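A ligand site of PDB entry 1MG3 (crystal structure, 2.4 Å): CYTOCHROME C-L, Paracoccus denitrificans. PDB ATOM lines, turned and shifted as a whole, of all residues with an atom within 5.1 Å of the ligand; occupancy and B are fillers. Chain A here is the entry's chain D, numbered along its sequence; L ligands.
A ring nitrogen (ND1) of His 61 lies within hydrogen-bond range of the backbone carbonyl oxygen (O) of Pro 71 (2.6 Å). The side-chain amide oxygen (OD1) of Asn 83 is in hydrogen-bond range of the side-chain hydroxyl (OG1) of Thr 92 (2.5 Å). The side-chain amide nitrogen of Asn 83 lies within hydrogen-bond range of the backbone carbonyl oxygen of Tyr 80. The side-chain amide oxygen (OD1) of Asn 83 lies close to the backbone NH (N) of Leu 89, at 3.5 Å. The backbone carbonyl oxygen (O) of Cys 60 is in hydrogen-bond range of the backbone NH (N) of Gly 70. The backbone carbonyl oxygen of Leu 93 lies within hydrogen-bond range of the backbone NH of Met 104 (2.7 Å).
Residues that only touch the ligand: Met 56, Pro 71, Leu 73, Trp 78, Leu 89, Thr 92, Leu 93, Ala 97 and Gln 100. Hydrophobic or aromatic side chains that line the ligand: Met 56, His 61, Pro 71, Leu 73, Trp 78, Tyr 80, Leu 89, Leu 93, Ala 97 and Met 101. 17 residues have an atom within 4 Å of the ligand: Met 56, Cys 57, Cys 60, His 61, Pro 71, Leu 73, Trp 78, Thr 79, Tyr 80, Asn 83, Leu 89, Thr 92, Leu 93, Ala 97, Thr 98, Gln 100 and Met 101.
An iron atom (FE1) of the ligand is bound by the side-chain sulfur of Met 101 (2.4 Å). The side-chain sulfur (SG) of Cys 57 is bonded to a carbon (C18) of the ligand, 1.8 Å away. SG of Cys 60 is bonded to C25 of the ligand. The backbone NH of Thr 79 sits close to an oxygen (O1) of the ligand, at 3.0 Å. A ring nitrogen (NE2) of His 61 binds an iron atom (FE1) of the ligand (2.1 Å). An oxygen (O1) of the ligand lies close to the backbone NH (N) of Tyr 80, at 3.0 Å. O3 of the ligand sits close to OH of Tyr 80 (3.5 Å). The side-chain amide nitrogen (ND2) of Asn 83 lies close to an oxygen (O1) of the ligand (3.0 Å). O3 of the ligand sits close to OG1 of Thr 98, at 2.4 Å. O2 of the ligand sits close to OG1 of Thr 79, 3.2 Å away.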
ATOM      1  N   TYR A  53      25.944  18.794  17.970  1.00  0.00           N
ATOM      2  CA  TYR A  53      25.240  19.974  18.450  1.00  0.00           C
ATOM      3  C   TYR A  53      26.102  21.226  18.309  1.00  0.00           C
ATOM      4  O   TYR A  53      25.586  22.334  18.142  1.00  0.00           O
ATOM      5  CB  TYR A  53      24.852  19.793  19.915  1.00  0.00           C
ATOM      6  CG  TYR A  53      24.236  21.033  20.520  1.00  0.00           C
ATOM      7  CD1 TYR A  53      22.896  21.335  20.302  1.00  0.00           C
ATOM      8  CD2 TYR A  53      25.012  21.934  21.222  1.00  0.00           C
ATOM      9  CE1 TYR A  53      22.340  22.525  20.761  1.00  0.00           C
ATOM     10  CE2 TYR A  53      24.483  23.139  21.685  1.00  0.00           C
ATOM     11  CZ  TYR A  53      23.144  23.431  21.453  1.00  0.00           C
ATOM     12  OH  TYR A  53      22.615  24.633  21.883  1.00  0.00           O
ATOM     13  N   MET A  56      26.088  22.109  14.483  1.00  0.00           N
ATOM     14  CA  MET A  56      24.787  21.949  13.856  1.00  0.00           C
ATOM     15  C   MET A  56      23.722  22.813  14.521  1.00  0.00           C
ATOM     16  O   MET A  56      22.738  23.178  13.881  1.00  0.00           O
ATOM     17  CB  MET A  56      24.386  20.468  13.904  1.00  0.00           C
ATOM     18  CG  MET A  56      23.453  19.985  12.803  1.00  0.00           C
ATOM     19  SD  MET A  56      24.202  19.960  11.160  1.00  0.00           S
ATOM     20  CE  MET A  56      23.081  21.067  10.267  1.00  0.00           C
ATOM     21  N   CYS A  57      23.908  23.144  15.801  1.00  0.00           N
ATOM     22  CA  CYS A  57      22.918  23.947  16.526  1.00  0.00           C
ATOM     23  C   CYS A  57      23.451  25.185  17.269  1.00  0.00           C
ATOM     24  O   CYS A  57      22.798  26.226  17.264  1.00  0.00           O
ATOM     25  CB  CYS A  57      22.181  23.061  17.538  1.00  0.00           C
ATOM     26  SG  CYS A  57      22.040  21.298  17.075  1.00  0.00           S
ATOM     27  N   CYS A  60      22.557  28.951  16.305  1.00  0.00           N
ATOM     28  CA  CYS A  60      21.319  29.646  16.607  1.00  0.00           C
ATOM     29  C   CYS A  60      20.895  29.470  18.074  1.00  0.00           C
ATOM     30  O   CYS A  60      20.413  30.415  18.687  1.00  0.00           O
ATOM     31  CB  CYS A  60      20.202  29.160  15.690  1.00  0.00           C
ATOM     32  SG  CYS A  60      20.416  29.482  13.898  1.00  0.00           S
ATOM     33  N   HIS A  61      21.093  28.277  18.632  1.00  0.00           N
ATOM     34  CA  HIS A  61      20.661  28.013  20.004  1.00  0.00           C
ATOM     35  C   HIS A  61      21.636  28.306  21.143  1.00  0.00           C
ATOM     36  O   HIS A  61      21.281  28.152  22.308  1.00  0.00           O
ATOM     37  CB  HIS A  61      20.136  26.583  20.116  1.00  0.00           C
ATOM     38  CG  HIS A  61      18.802  26.386  19.445  1.00  0.00           C
ATOM     39  ND1 HIS A  61      17.717  27.118  19.841  1.00  0.00           N
ATOM     40  CD2 HIS A  61      18.704  25.505  18.435  1.00  0.00           C
ATOM     41  CE1 HIS A  61      16.776  26.661  18.940  1.00  0.00           C
ATOM     42  NE2 HIS A  61      17.352  25.670  18.074  1.00  0.00           N
ATOM     43  N   GLY A  70      18.289  32.012  18.568  1.00  0.00           N
ATOM     44  CA  GLY A  70      17.091  31.210  18.709  1.00  0.00           C
ATOM     45  C   GLY A  70      16.786  30.956  20.166  1.00  0.00           C
ATOM     46  O   GLY A  70      17.546  31.374  21.058  1.00  0.00           O
ATOM     47  N   PRO A  71      15.680  30.257  20.458  1.00  0.00           N
ATOM     48  CA  PRO A  71      15.217  29.932  21.809  1.00  0.00           C
ATOM     49  C   PRO A  71      16.133  29.004  22.601  1.00  0.00           C
ATOM     50  O   PRO A  71      17.047  28.381  22.058  1.00  0.00           O
ATOM     51  CB  PRO A  71      13.841  29.312  21.552  1.00  0.00           C
ATOM     52  CG  PRO A  71      14.050  28.608  20.256  1.00  0.00           C
ATOM     53  CD  PRO A  71      14.821  29.622  19.438  1.00  0.00           C
ATOM     54  N   GLY A  72      15.874  28.914  23.903  1.00  0.00           N
ATOM     55  CA  GLY A  72      16.679  28.066  24.769  1.00  0.00           C
ATOM     56  C   GLY A  72      16.153  26.646  24.725  1.00  0.00           C
ATOM     57  O   GLY A  72      14.955  26.443  24.537  1.00  0.00           O
ATOM     58  N   LEU A  73      17.050  25.682  24.879  1.00  0.00           N
ATOM     59  CA  LEU A  73      16.680  24.266  24.854  1.00  0.00           C
ATOM     60  C   LEU A  73      17.165  23.549  26.094  1.00  0.00           C
ATOM     61  O   LEU A  73      17.080  22.323  26.181  1.00  0.00           O
ATOM     62  CB  LEU A  73      17.298  23.580  23.628  1.00  0.00           C
ATOM     63  CG  LEU A  73      16.696  23.728  22.232  1.00  0.00           C
ATOM     64  CD1 LEU A  73      16.222  25.146  21.984  1.00  0.00           C
ATOM     65  CD2 LEU A  73      17.741  23.338  21.206  1.00  0.00           C
ATOM     66  N   TRP A  78       9.056  24.312  27.146  1.00  0.00           N
ATOM     67  CA  TRP A  78       9.106  23.947  25.731  1.00  0.00           C
ATOM     68  C   TRP A  78       7.914  24.545  25.010  1.00  0.00           C
ATOM     69  O   TRP A  78       6.769  24.304  25.380  1.00  0.00           O
ATOM     70  CB  TRP A  78       9.090  22.420  25.561  1.00  0.00           C
ATOM     71  CG  TRP A  78      10.296  21.714  26.106  1.00  0.00           C
ATOM     72  CD1 TRP A  78      10.381  21.035  27.285  1.00  0.00           C
ATOM     73  CD2 TRP A  78      11.574  21.556  25.464  1.00  0.00           C
ATOM     74  NE1 TRP A  78      11.620  20.449  27.415  1.00  0.00           N
ATOM     75  CE2 TRP A  78      12.376  20.761  26.306  1.00  0.00           C
ATOM     76  CE3 TRP A  78      12.114  22.004  24.249  1.00  0.00           C
ATOM     77  CZ2 TRP A  78      13.690  20.395  25.981  1.00  0.00           C
ATOM     78  CZ3 TRP A  78      13.429  21.641  23.915  1.00  0.00           C
ATOM     79  CH2 TRP A  78      14.201  20.851  24.781  1.00  0.00           C
ATOM     80  N   THR A  79       8.197  25.338  23.978  1.00  0.00           N
ATOM     81  CA  THR A  79       7.138  25.965  23.178  1.00  0.00           C
ATOM     82  C   THR A  79       6.248  24.869  22.622  1.00  0.00           C
ATOM     83  O   THR A  79       5.032  25.035  22.470  1.00  0.00           O
ATOM     84  CB  THR A  79       7.743  26.801  22.047  1.00  0.00           C
ATOM     85  OG1 THR A  79       8.462  27.912  22.613  1.00  0.00           O
ATOM     86  CG2 THR A  79       6.664  27.313  21.101  1.00  0.00           C
ATOM     87  N   TYR A  80       6.872  23.736  22.310  1.00  0.00           N
ATOM     88  CA  TYR A  80       6.157  22.572  21.810  1.00  0.00           C
ATOM     89  C   TYR A  80       6.316  21.551  22.929  1.00  0.00           C
ATOM     90  O   TYR A  80       7.257  20.761  22.942  1.00  0.00           O
ATOM     91  CB  TYR A  80       6.789  22.097  20.499  1.00  0.00           C
ATOM     92  CG  TYR A  80       6.616  23.123  19.403  1.00  0.00           C
ATOM     93  CD1 TYR A  80       5.365  23.358  18.841  1.00  0.00           C
ATOM     94  CD2 TYR A  80       7.687  23.920  18.999  1.00  0.00           C
ATOM     95  CE1 TYR A  80       5.180  24.360  17.896  1.00  0.00           C
ATOM     96  CE2 TYR A  80       7.515  24.939  18.049  1.00  0.00           C
ATOM     97  CZ  TYR A  80       6.252  25.150  17.510  1.00  0.00           C
ATOM     98  OH  TYR A  80       6.059  26.161  16.600  1.00  0.00           O
ATOM     99  N   ASN A  83       8.259  18.173  23.302  1.00  0.00           N
ATOM    100  CA  ASN A  83       9.710  18.100  23.364  1.00  0.00           C
ATOM    101  C   ASN A  83      10.268  17.671  24.715  1.00  0.00           C
ATOM    102  O   ASN A  83      11.483  17.521  24.862  1.00  0.00           O
ATOM    103  CB  ASN A  83      10.325  19.436  22.941  1.00  0.00           C
ATOM    104  CG  ASN A  83      10.146  19.714  21.452  1.00  0.00           C
ATOM    105  OD1 ASN A  83      10.389  18.841  20.616  1.00  0.00           O
ATOM    106  ND2 ASN A  83       9.743  20.927  21.118  1.00  0.00           N
ATOM    107  N   LEU A  89      10.644  15.366  20.745  1.00  0.00           N
ATOM    108  CA  LEU A  89      11.865  16.047  20.359  1.00  0.00           C
ATOM    109  C   LEU A  89      12.307  15.545  18.981  1.00  0.00           C
ATOM    110  O   LEU A  89      12.705  16.320  18.109  1.00  0.00           O
ATOM    111  CB  LEU A  89      12.971  15.767  21.376  1.00  0.00           C
ATOM    112  CG  LEU A  89      14.015  16.871  21.602  1.00  0.00           C
ATOM    113  CD1 LEU A  89      15.128  16.285  22.468  1.00  0.00           C
ATOM    114  CD2 LEU A  89      14.557  17.396  20.277  1.00  0.00           C
ATOM    115  N   THR A  92      10.275  16.854  16.209  1.00  0.00           N
ATOM    116  CA  THR A  92      10.609  18.261  15.978  1.00  0.00           C
ATOM    117  C   THR A  92      11.758  18.412  14.971  1.00  0.00           C
ATOM    118  O   THR A  92      11.654  19.175  14.013  1.00  0.00           O
ATOM    119  CB  THR A  92      11.009  18.987  17.286  1.00  0.00           C
ATOM    120  OG1 THR A  92       9.855  19.099  18.143  1.00  0.00           O
ATOM    121  CG2 THR A  92      11.550  20.375  17.000  1.00  0.00           C
ATOM    122  N   LEU A  93      12.858  17.696  15.207  1.00  0.00           N
ATOM    123  CA  LEU A  93      14.006  17.767  14.320  1.00  0.00           C
ATOM    124  C   LEU A  93      13.671  17.229  12.939  1.00  0.00           C
ATOM    125  O   LEU A  93      13.929  17.870  11.928  1.00  0.00           O
ATOM    126  CB  LEU A  93      15.183  16.959  14.872  1.00  0.00           C
ATOM    127  CG  LEU A  93      15.643  17.332  16.276  1.00  0.00           C
ATOM    128  CD1 LEU A  93      17.011  16.728  16.524  1.00  0.00           C
ATOM    129  CD2 LEU A  93      15.703  18.826  16.423  1.00  0.00           C
ATOM    130  N   ALA A  97       9.800  22.859  12.462  1.00  0.00           N
ATOM    131  CA  ALA A  97       8.899  23.718  13.237  1.00  0.00           C
ATOM    132  C   ALA A  97       8.384  24.873  12.366  1.00  0.00           C
ATOM    133  O   ALA A  97       7.516  24.681  11.515  1.00  0.00           O
ATOM    134  CB  ALA A  97       9.636  24.274  14.454  1.00  0.00           C
ATOM    135  N   THR A  98       8.918  26.073  12.586  1.00  0.00           N
ATOM    136  CA  THR A  98       8.551  27.258  11.806  1.00  0.00           C
ATOM    137  C   THR A  98       9.771  28.165  11.671  1.00  0.00           C
ATOM    138  O   THR A  98      10.660  28.155  12.524  1.00  0.00           O
ATOM    139  CB  THR A  98       7.426  28.078  12.478  1.00  0.00           C
ATOM    140  OG1 THR A  98       7.990  28.877  13.531  1.00  0.00           O
ATOM    141  CG2 THR A  98       6.348  27.173  13.057  1.00  0.00           C
ATOM    142  N   GLN A 100      13.312  29.492  10.549  1.00  0.00           N
ATOM    143  CA  GLN A 100      14.596  28.853  10.245  1.00  0.00           C
ATOM    144  C   GLN A 100      14.763  27.486  10.902  1.00  0.00           C
ATOM    145  O   GLN A 100      15.890  26.983  11.011  1.00  0.00           O
ATOM    146  CB  GLN A 100      15.752  29.784  10.639  1.00  0.00           C
ATOM    147  CG  GLN A 100      15.930  30.968   9.696  1.00  0.00           C
ATOM    148  CD  GLN A 100      17.140  31.823  10.041  1.00  0.00           C
ATOM    149  OE1 GLN A 100      17.184  32.455  11.103  1.00  0.00           O
ATOM    150  NE2 GLN A 100      18.122  31.836   9.159  1.00  0.00           N
ATOM    151  N   MET A 101      13.658  26.884  11.323  1.00  0.00           N
ATOM    152  CA  MET A 101      13.686  25.572  11.950  1.00  0.00           C
ATOM    153  C   MET A 101      12.828  24.625  11.107  1.00  0.00           C
ATOM    154  O   MET A 101      11.663  24.370  11.409  1.00  0.00           O
ATOM    155  CB  MET A 101      13.132  25.641  13.380  1.00  0.00           C
ATOM    156  CG  MET A 101      13.322  24.366  14.207  1.00  0.00           C
ATOM    157  SD  MET A 101      15.058  23.978  14.638  1.00  0.00           S
ATOM    158  CE  MET A 101      15.172  22.309  14.064  1.00  0.00           C
ATOM    159  N   MET A 104      14.961  18.331   9.463  1.00  0.00           N
ATOM    160  CA  MET A 104      16.352  17.896   9.473  1.00  0.00           C
ATOM    161  C   MET A 104      16.597  16.578   8.744  1.00  0.00           C
ATOM    162  O   MET A 104      17.747  16.143   8.622  1.00  0.00           O
ATOM    163  CB  MET A 104      16.850  17.717  10.914  1.00  0.00           C
ATOM    164  CG  MET A 104      16.901  18.959  11.767  1.00  0.00           C
ATOM    165  SD  MET A 104      18.292  20.041  11.381  1.00  0.00           S
ATOM    166  CE  MET A 104      17.423  21.513  10.759  1.00  0.00           C
ATOM    167  N   LEU A 108      20.619  15.413   8.562  1.00  0.00           N
ATOM    168  CA  LEU A 108      20.971  14.460   9.615  1.00  0.00           C
ATOM    169  C   LEU A 108      20.400  13.071   9.350  1.00  0.00           C
ATOM    170  O   LEU A 108      19.338  12.932   8.756  1.00  0.00           O
ATOM    171  CB  LEU A 108      20.471  14.967  10.965  1.00  0.00           C
ATOM    172  CG  LEU A 108      21.062  16.283  11.480  1.00  0.00           C
ATOM    173  CD1 LEU A 108      20.266  16.761  12.690  1.00  0.00           C
ATOM    174  CD2 LEU A 108      22.537  16.081  11.825  1.00  0.00           C
ATOM    175  N   THR A 116      22.589  13.839  18.649  1.00  0.00           N
ATOM    176  CA  THR A 116      22.476  15.270  18.916  1.00  0.00           C
ATOM    177  C   THR A 116      21.442  15.511  20.027  1.00  0.00           C
ATOM    178  O   THR A 116      21.664  16.326  20.925  1.00  0.00           O
ATOM    179  CB  THR A 116      22.058  16.036  17.638  1.00  0.00           C
ATOM    180  OG1 THR A 116      22.957  15.713  16.565  1.00  0.00           O
ATOM    181  CG2 THR A 116      22.097  17.532  17.881  1.00  0.00           C
ATOM    182  N   VAL A 120      21.590  17.488  23.770  1.00  0.00           N
ATOM    183  CA  VAL A 120      20.668  18.540  24.147  1.00  0.00           C
ATOM    184  C   VAL A 120      20.105  18.230  25.517  1.00  0.00           C
ATOM    185  O   VAL A 120      19.860  19.131  26.321  1.00  0.00           O
ATOM    186  CB  VAL A 120      19.488  18.660  23.139  1.00  0.00           C
ATOM    187  CG1 VAL A 120      18.373  19.521  23.740  1.00  0.00           C
ATOM    188  CG2 VAL A 120      19.973  19.281  21.850  1.00  0.00           C
HETATM  189 FE1  LIG L   1      16.314  24.836  16.458  1.00  0.00          FE
HETATM  190  C1  LIG L   1      13.293  25.630  17.724  1.00  0.00           C
HETATM  191  C2  LIG L   1      16.227  21.860  18.121  1.00  0.00           C
HETATM  192  C3  LIG L   1      19.367  24.004  15.178  1.00  0.00           C
HETATM  193  C4  LIG L   1      16.473  27.804  14.832  1.00  0.00           C
HETATM  194  N1  LIG L   1      14.992  23.913  17.695  1.00  0.00           N
HETATM  195  C5  LIG L   1      13.789  24.417  18.097  1.00  0.00           C
HETATM  196  C6  LIG L   1      13.149  23.456  18.983  1.00  0.00           C
HETATM  197  C7  LIG L   1      13.974  22.393  19.083  1.00  0.00           C
HETATM  198  C8  LIG L   1      15.144  22.666  18.288  1.00  0.00           C
HETATM  199  C9  LIG L   1      13.767  21.108  19.906  1.00  0.00           C
HETATM  200  C10 LIG L   1      11.789  23.671  19.638  1.00  0.00           C
HETATM  201  C11 LIG L   1      11.974  24.018  21.125  1.00  0.00           C
HETATM  202  C12 LIG L   1      10.758  24.608  21.813  1.00  0.00           C
HETATM  203  O1  LIG L   1       9.832  23.768  22.071  1.00  0.00           O
HETATM  204  O2  LIG L   1      10.754  25.803  22.068  1.00  0.00           O
HETATM  205  N2  LIG L   1      17.558  23.258  16.607  1.00  0.00           N
HETATM  206  C13 LIG L   1      17.341  22.115  17.365  1.00  0.00           C
HETATM  207  C14 LIG L   1      18.481  21.209  17.214  1.00  0.00           C
HETATM  208  C15 LIG L   1      19.344  21.818  16.388  1.00  0.00           C
HETATM  209  C16 LIG L   1      18.788  23.087  16.014  1.00  0.00           C
HETATM  210  C17 LIG L   1      18.613  19.837  17.902  1.00  0.00           C
HETATM  211  C18 LIG L   1      20.702  21.339  15.862  1.00  0.00           C
HETATM  212  C19 LIG L   1      20.612  20.138  14.908  1.00  0.00           C
HETATM  213  N3  LIG L   1      17.639  25.732  15.254  1.00  0.00           N
HETATM  214  C20 LIG L   1      18.849  25.225  14.840  1.00  0.00           C
HETATM  215  C21 LIG L   1      19.546  26.181  13.982  1.00  0.00           C
HETATM  216  C22 LIG L   1      18.756  27.249  13.894  1.00  0.00           C
HETATM  217  C23 LIG L   1      17.558  26.981  14.670  1.00  0.00           C
HETATM  218  C24 LIG L   1      20.945  25.918  13.362  1.00  0.00           C
HETATM  219  C25 LIG L   1      19.018  28.558  13.141  1.00  0.00           C
HETATM  220  C26 LIG L   1      19.065  28.448  11.604  1.00  0.00           C
HETATM  221  N4  LIG L   1      15.129  26.392  16.299  1.00  0.00           N
HETATM  222  C27 LIG L   1      15.351  27.561  15.572  1.00  0.00           C
HETATM  223  C28 LIG L   1      14.219  28.461  15.721  1.00  0.00           C
HETATM  224  C29 LIG L   1      13.327  27.853  16.537  1.00  0.00           C
HETATM  225  C30 LIG L   1      13.892  26.569  16.894  1.00  0.00           C
HETATM  226  C31 LIG L   1      14.106  29.858  15.073  1.00  0.00           C
HETATM  227  C32 LIG L   1      11.980  28.391  16.987  1.00  0.00           C
HETATM  228  C33 LIG L   1      10.843  27.592  16.268  1.00  0.00           C
HETATM  229  C34 LIG L   1       9.473  28.037  16.675  1.00  0.00           C
HETATM  230  O3  LIG L   1       8.644  28.309  15.796  1.00  0.00           O
HETATM  231  O4  LIG L   1       9.274  28.095  17.911  1.00  0.00           O
